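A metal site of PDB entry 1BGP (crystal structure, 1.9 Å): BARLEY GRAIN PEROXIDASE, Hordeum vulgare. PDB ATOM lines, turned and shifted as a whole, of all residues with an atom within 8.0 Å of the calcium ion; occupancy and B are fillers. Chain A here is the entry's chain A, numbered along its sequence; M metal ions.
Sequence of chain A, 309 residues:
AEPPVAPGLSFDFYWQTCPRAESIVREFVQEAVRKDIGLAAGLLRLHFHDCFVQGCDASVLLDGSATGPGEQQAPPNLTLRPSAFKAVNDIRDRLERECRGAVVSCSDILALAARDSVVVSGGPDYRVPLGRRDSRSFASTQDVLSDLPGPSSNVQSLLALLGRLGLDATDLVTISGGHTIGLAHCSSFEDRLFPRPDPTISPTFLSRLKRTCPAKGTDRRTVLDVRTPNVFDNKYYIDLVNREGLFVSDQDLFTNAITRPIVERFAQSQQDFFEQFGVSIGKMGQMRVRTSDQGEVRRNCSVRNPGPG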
ATOM      1  N   SER A 121      25.099  10.128 -15.585  1.00  0.00           N
ATOM      2  CA  SER A 121      24.339   9.153 -16.358  1.00  0.00           C
ATOM      3  C   SER A 121      25.133   7.879 -16.664  1.00  0.00           C
ATOM      4  O   SER A 121      24.665   7.032 -17.438  1.00  0.00           O
ATOM      5  CB  SER A 121      23.815   9.794 -17.648  1.00  0.00           C
ATOM      6  OG  SER A 121      22.949  10.875 -17.357  1.00  0.00           O
ATOM      7  N   GLY A 177      26.404  10.787 -30.263  1.00  0.00           N
ATOM      8  CA  GLY A 177      26.207   9.794 -29.221  1.00  0.00           C
ATOM      9  C   GLY A 177      25.438  10.378 -28.044  1.00  0.00           C
ATOM     10  O   GLY A 177      25.040   9.649 -27.137  1.00  0.00           O
ATOM     11  N   GLY A 178      25.264  11.697 -28.050  1.00  0.00           N
ATOM     12  CA  GLY A 178      24.501  12.340 -26.985  1.00  0.00           C
ATOM     13  C   GLY A 178      23.075  11.812 -26.976  1.00  0.00           C
ATOM     14  O   GLY A 178      22.400  11.872 -25.952  1.00  0.00           O
ATOM     15  N   HIS A 179      22.643  11.259 -28.101  1.00  0.00           N
ATOM     16  CA  HIS A 179      21.291  10.693 -28.215  1.00  0.00           C
ATOM     17  C   HIS A 179      21.155   9.342 -27.521  1.00  0.00           C
ATOM     18  O   HIS A 179      20.182   8.622 -27.729  1.00  0.00           O
ATOM     19  CB  HIS A 179      20.875  10.584 -29.685  1.00  0.00           C
ATOM     20  CG  HIS A 179      20.698  11.989 -30.226  1.00  0.00           C
ATOM     21  ND1 HIS A 179      20.534  12.242 -31.585  1.00  0.00           N
ATOM     22  CD2 HIS A 179      20.593  13.180 -29.517  1.00  0.00           C
ATOM     23  CE1 HIS A 179      20.284  13.553 -31.709  1.00  0.00           C
ATOM     24  NE2 HIS A 179      20.316  14.095 -30.526  1.00  0.00           N
ATOM     25  N   THR A 180      22.153   8.976 -26.719  1.00  0.00           N
ATOM     26  CA  THR A 180      22.091   7.740 -25.981  1.00  0.00           C
ATOM     27  C   THR A 180      21.184   7.928 -24.766  1.00  0.00           C
ATOM     28  O   THR A 180      20.943   6.983 -24.008  1.00  0.00           O
ATOM     29  CB  THR A 180      23.491   7.259 -25.553  1.00  0.00           C
ATOM     30  OG1 THR A 180      23.409   5.926 -25.032  1.00  0.00           O
ATOM     31  CG2 THR A 180      24.086   8.184 -24.502  1.00  0.00           C
ATOM     32  N   ILE A 181      20.725   9.163 -24.552  1.00  0.00           N
ATOM     33  CA  ILE A 181      19.815   9.488 -23.457  1.00  0.00           C
ATOM     34  C   ILE A 181      18.864  10.571 -23.973  1.00  0.00           C
ATOM     35  O   ILE A 181      19.117  11.161 -25.033  1.00  0.00           O
ATOM     36  CB  ILE A 181      20.537  10.058 -22.209  1.00  0.00           C
ATOM     37  CG1 ILE A 181      21.300  11.338 -22.544  1.00  0.00           C
ATOM     38  CG2 ILE A 181      21.437   8.999 -21.594  1.00  0.00           C
ATOM     39  CD1 ILE A 181      21.775  12.095 -21.329  1.00  0.00           C
ATOM     40  N   GLY A 182      17.775  10.807 -23.265  1.00  0.00           N
ATOM     41  CA  GLY A 182      16.851  11.849 -23.688  1.00  0.00           C
ATOM     42  C   GLY A 182      15.618  11.419 -24.449  1.00  0.00           C
ATOM     43  O   GLY A 182      15.426  10.245 -24.778  1.00  0.00           O
ATOM     44  N   LEU A 224      15.149   8.527 -27.373  1.00  0.00           N
ATOM     45  CA  LEU A 224      16.082   8.567 -28.482  1.00  0.00           C
ATOM     46  C   LEU A 224      16.828   7.245 -28.609  1.00  0.00           C
ATOM     47  O   LEU A 224      17.146   6.807 -29.720  1.00  0.00           O
ATOM     48  CB  LEU A 224      17.065   9.721 -28.285  1.00  0.00           C
ATOM     49  CG  LEU A 224      16.525  11.117 -28.577  1.00  0.00           C
ATOM     50  CD1 LEU A 224      17.390  12.165 -27.902  1.00  0.00           C
ATOM     51  CD2 LEU A 224      16.472  11.357 -30.078  1.00  0.00           C
ATOM     52  N   ASP A 225      17.085   6.611 -27.472  1.00  0.00           N
ATOM     53  CA  ASP A 225      17.780   5.328 -27.417  1.00  0.00           C
ATOM     54  C   ASP A 225      16.814   4.288 -26.875  1.00  0.00           C
ATOM     55  O   ASP A 225      16.629   4.171 -25.661  1.00  0.00           O
ATOM     56  CB  ASP A 225      19.009   5.438 -26.504  1.00  0.00           C
ATOM     57  CG  ASP A 225      19.810   4.139 -26.409  1.00  0.00           C
ATOM     58  OD1 ASP A 225      19.360   3.076 -26.894  1.00  0.00           O
ATOM     59  OD2 ASP A 225      20.907   4.184 -25.842  1.00  0.00           O
ATOM     60  N   VAL A 226      16.259   3.491 -27.776  1.00  0.00           N
ATOM     61  CA  VAL A 226      15.297   2.466 -27.404  1.00  0.00           C
ATOM     62  C   VAL A 226      15.843   1.417 -26.427  1.00  0.00           C
ATOM     63  O   VAL A 226      15.088   0.872 -25.617  1.00  0.00           O
ATOM     64  CB  VAL A 226      14.688   1.795 -28.667  1.00  0.00           C
ATOM     65  CG1 VAL A 226      15.727   0.949 -29.400  1.00  0.00           C
ATOM     66  CG2 VAL A 226      13.476   0.981 -28.294  1.00  0.00           C
ATOM     67  N   ARG A 227      17.147   1.143 -26.486  1.00  0.00           N
ATOM     68  CA  ARG A 227      17.764   0.153 -25.606  1.00  0.00           C
ATOM     69  C   ARG A 227      17.979   0.625 -24.163  1.00  0.00           C
ATOM     70  O   ARG A 227      17.500  -0.015 -23.226  1.00  0.00           O
ATOM     71  CB  ARG A 227      19.050  -0.376 -26.223  1.00  0.00           C
ATOM     72  CG  ARG A 227      18.776  -1.340 -27.375  1.00  0.00           C
ATOM     73  CD  ARG A 227      20.006  -1.727 -28.159  1.00  0.00           C
ATOM     74  NE  ARG A 227      19.690  -2.741 -29.154  1.00  0.00           N
ATOM     75  CZ  ARG A 227      19.023  -2.519 -30.287  1.00  0.00           C
ATOM     76  NH1 ARG A 227      18.603  -1.303 -30.587  1.00  0.00           N
ATOM     77  NH2 ARG A 227      18.721  -3.528 -31.089  1.00  0.00           N
ATOM     78  N   THR A 228      18.722   1.713 -23.970  1.00  0.00           N
ATOM     79  CA  THR A 228      18.939   2.231 -22.622  1.00  0.00           C
ATOM     80  C   THR A 228      18.629   3.730 -22.630  1.00  0.00           C
ATOM     81  O   THR A 228      19.546   4.560 -22.735  1.00  0.00           O
ATOM     82  CB  THR A 228      20.377   1.985 -22.118  1.00  0.00           C
ATOM     83  OG1 THR A 228      21.329   2.482 -23.072  1.00  0.00           O
ATOM     84  CG2 THR A 228      20.608   0.502 -21.868  1.00  0.00           C
ATOM     85  N   PRO A 229      17.339   4.088 -22.537  1.00  0.00           N
ATOM     86  CA  PRO A 229      16.851   5.465 -22.542  1.00  0.00           C
ATOM     87  C   PRO A 229      17.568   6.468 -21.639  1.00  0.00           C
ATOM     88  O   PRO A 229      17.845   7.594 -22.066  1.00  0.00           O
ATOM     89  CB  PRO A 229      15.392   5.307 -22.135  1.00  0.00           C
ATOM     90  CG  PRO A 229      15.028   3.990 -22.749  1.00  0.00           C
ATOM     91  CD  PRO A 229      16.223   3.145 -22.375  1.00  0.00           C
ATOM     92  N   ASN A 230      17.891   6.072 -20.417  1.00  0.00           N
ATOM     93  CA  ASN A 230      18.528   6.977 -19.463  1.00  0.00           C
ATOM     94  C   ASN A 230      19.979   6.712 -19.085  1.00  0.00           C
ATOM     95  O   ASN A 230      20.520   7.388 -18.213  1.00  0.00           O
ATOM     96  CB  ASN A 230      17.689   7.051 -18.191  1.00  0.00           C
ATOM     97  CG  ASN A 230      16.252   7.417 -18.462  1.00  0.00           C
ATOM     98  OD1 ASN A 230      15.960   8.264 -19.309  1.00  0.00           O
ATOM     99  ND2 ASN A 230      15.336   6.743 -17.793  1.00  0.00           N
ATOM    100  N   VAL A 231      20.603   5.727 -19.718  1.00  0.00           N
ATOM    101  CA  VAL A 231      21.998   5.397 -19.407  1.00  0.00           C
ATOM    102  C   VAL A 231      22.908   5.893 -20.521  1.00  0.00           C
ATOM    103  O   VAL A 231      22.649   5.630 -21.703  1.00  0.00           O
ATOM    104  CB  VAL A 231      22.197   3.872 -19.243  1.00  0.00           C
ATOM    105  CG1 VAL A 231      23.655   3.567 -18.882  1.00  0.00           C
ATOM    106  CG2 VAL A 231      21.274   3.330 -18.166  1.00  0.00           C
ATOM    107  N   PHE A 232      23.957   6.628 -20.154  1.00  0.00           N
ATOM    108  CA  PHE A 232      24.901   7.122 -21.138  1.00  0.00           C
ATOM    109  C   PHE A 232      25.850   5.975 -21.466  1.00  0.00           C
ATOM    110  O   PHE A 232      26.675   5.580 -20.636  1.00  0.00           O
ATOM    111  CB  PHE A 232      25.686   8.327 -20.614  1.00  0.00           C
ATOM    112  CG  PHE A 232      26.495   9.022 -21.678  1.00  0.00           C
ATOM    113  CD1 PHE A 232      27.739   8.544 -22.051  1.00  0.00           C
ATOM    114  CD2 PHE A 232      25.967  10.122 -22.344  1.00  0.00           C
ATOM    115  CE1 PHE A 232      28.454   9.128 -23.085  1.00  0.00           C
ATOM    116  CE2 PHE A 232      26.671  10.727 -23.385  1.00  0.00           C
ATOM    117  CZ  PHE A 232      27.920  10.221 -23.762  1.00  0.00           C
ATOM    118  N   ASP A 233      25.746   5.462 -22.679  1.00  0.00           N
ATOM    119  CA  ASP A 233      26.559   4.324 -23.117  1.00  0.00           C
ATOM    120  C   ASP A 233      26.562   4.272 -24.639  1.00  0.00           C
ATOM    121  O   ASP A 233      25.934   5.108 -25.280  1.00  0.00           O
ATOM    122  CB  ASP A 233      25.990   3.028 -22.524  1.00  0.00           C
ATOM    123  CG  ASP A 233      24.506   2.851 -22.789  1.00  0.00           C
ATOM    124  OD1 ASP A 233      23.960   3.457 -23.737  1.00  0.00           O
ATOM    125  OD2 ASP A 233      23.855   2.095 -22.041  1.00  0.00           O
ATOM    126  N   ASN A 234      27.162   3.235 -25.208  1.00  0.00           N
ATOM    127  CA  ASN A 234      27.234   3.102 -26.657  1.00  0.00           C
ATOM    128  C   ASN A 234      26.014   2.445 -27.313  1.00  0.00           C
ATOM    129  O   ASN A 234      26.003   2.234 -28.525  1.00  0.00           O
ATOM    130  CB  ASN A 234      28.496   2.335 -27.067  1.00  0.00           C
ATOM    131  CG  ASN A 234      28.403   0.861 -26.752  1.00  0.00           C
ATOM    132  OD1 ASN A 234      27.664   0.444 -25.861  1.00  0.00           O
ATOM    133  ND2 ASN A 234      29.139   0.057 -27.505  1.00  0.00           N
ATOM    134  N   LYS A 235      24.981   2.145 -26.524  1.00  0.00           N
ATOM    135  CA  LYS A 235      23.777   1.500 -27.069  1.00  0.00           C
ATOM    136  C   LYS A 235      23.157   2.256 -28.241  1.00  0.00           C
ATOM    137  O   LYS A 235      22.485   1.667 -29.080  1.00  0.00           O
ATOM    138  CB  LYS A 235      22.737   1.268 -25.973  1.00  0.00           C
ATOM    139  CG  LYS A 235      23.140   0.225 -24.933  1.00  0.00           C
ATOM    140  CD  LYS A 235      23.436  -1.119 -25.570  1.00  0.00           C
ATOM    141  CE  LYS A 235      23.800  -2.182 -24.540  1.00  0.00           C
ATOM    142  NZ  LYS A 235      25.028  -1.847 -23.784  1.00  0.00           N
ATOM    143  N   TYR A 236      23.415   3.562 -28.302  1.00  0.00           N
ATOM    144  CA  TYR A 236      22.907   4.390 -29.389  1.00  0.00           C
ATOM    145  C   TYR A 236      23.448   3.908 -30.726  1.00  0.00           C
ATOM    146  O   TYR A 236      22.731   3.855 -31.718  1.00  0.00           O
ATOM    147  CB  TYR A 236      23.305   5.859 -29.149  1.00  0.00           C
ATOM    148  CG  TYR A 236      23.234   6.743 -30.392  1.00  0.00           C
ATOM    149  CD1 TYR A 236      22.005   7.220 -30.864  1.00  0.00           C
ATOM    150  CD2 TYR A 236      24.392   7.093 -31.081  1.00  0.00           C
ATOM    151  CE1 TYR A 236      21.939   8.028 -31.998  1.00  0.00           C
ATOM    152  CE2 TYR A 236      24.331   7.909 -32.213  1.00  0.00           C
ATOM    153  CZ  TYR A 236      23.107   8.367 -32.658  1.00  0.00           C
ATOM    154  OH  TYR A 236      23.070   9.175 -33.763  1.00  0.00           O
ATOM    155  N   TYR A 237      24.729   3.536 -30.749  1.00  0.00           N
ATOM    156  CA  TYR A 237      25.353   3.056 -31.970  1.00  0.00           C
ATOM    157  C   TYR A 237      24.815   1.687 -32.346  1.00  0.00           C
ATOM    158  O   TYR A 237      24.622   1.379 -33.530  1.00  0.00           O
ATOM    159  CB  TYR A 237      26.875   3.046 -31.810  1.00  0.00           C
ATOM    160  CG  TYR A 237      27.406   4.431 -31.532  1.00  0.00           C
ATOM    161  CD1 TYR A 237      27.513   5.375 -32.555  1.00  0.00           C
ATOM    162  CD2 TYR A 237      27.724   4.824 -30.242  1.00  0.00           C
ATOM    163  CE1 TYR A 237      27.922   6.676 -32.302  1.00  0.00           C
ATOM    164  CE2 TYR A 237      28.141   6.130 -29.969  1.00  0.00           C
ATOM    165  CZ  TYR A 237      28.230   7.050 -30.995  1.00  0.00           C
ATOM    166  OH  TYR A 237      28.617   8.354 -30.740  1.00  0.00           O
ATOM    167  N   ASP A 239      21.845   0.808 -31.752  1.00  0.00           N
ATOM    168  CA  ASP A 239      20.519   1.104 -32.297  1.00  0.00           C
ATOM    169  C   ASP A 239      20.672   1.361 -33.801  1.00  0.00           C
ATOM    170  O   ASP A 239      19.930   0.804 -34.609  1.00  0.00           O
ATOM    171  CB  ASP A 239      19.904   2.377 -31.679  1.00  0.00           C
ATOM    172  CG  ASP A 239      19.643   2.258 -30.196  1.00  0.00           C
ATOM    173  OD1 ASP A 239      19.375   1.143 -29.698  1.00  0.00           O
ATOM    174  OD2 ASP A 239      19.680   3.306 -29.521  1.00  0.00           O
ATOM    175  N   GLN A 270      32.597   0.297 -26.278  1.00  0.00           N
ATOM    176  CA  GLN A 270      32.109   1.457 -25.546  1.00  0.00           C
ATOM    177  C   GLN A 270      33.292   2.300 -25.110  1.00  0.00           C
ATOM    178  O   GLN A 270      33.221   3.532 -25.098  1.00  0.00           O
ATOM    179  CB  GLN A 270      31.293   1.021 -24.338  1.00  0.00           C
ATOM    180  CG  GLN A 270      30.870   2.180 -23.448  1.00  0.00           C
ATOM    181  CD  GLN A 270      29.684   1.830 -22.584  1.00  0.00           C
ATOM    182  OE1 GLN A 270      28.571   1.703 -23.072  1.00  0.00           O
ATOM    183  NE2 GLN A 270      29.908   1.701 -21.281  1.00  0.00           N
HETATM  184 CA    CA M   1      21.678   4.820 -23.632  1.00  0.00          CA
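The calcium ion is bound by O of Val 231 (2.3 Å), O of Thr 180 (2.3 Å), O of Thr 228 (2.3 Å), OD2 of Asp 225 (2.4 Å), OG1 of Thr 228 (2.4 Å), OG1 of Thr 180 (2.5 Å) and OD1 of Asp 233 (2.7 Å). The calcium ion has seven donor atoms within binding distance.
OD1 of Asp 225 sits at hydrogen-bond distance from N of Arg 227 (3.0 Å). OD2 of Asp 239 lies close to OD1 of Asp 225 (2.7 Å). The side-chain carboxylate (OD1) of Asp 233 lies close to the backbone NH (N) of Lys 235, at 3.2 Å.
Within 4 Å of the calcium ion: Thr 180, Asp 225, Thr 228, Val 231 and Asp 233.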
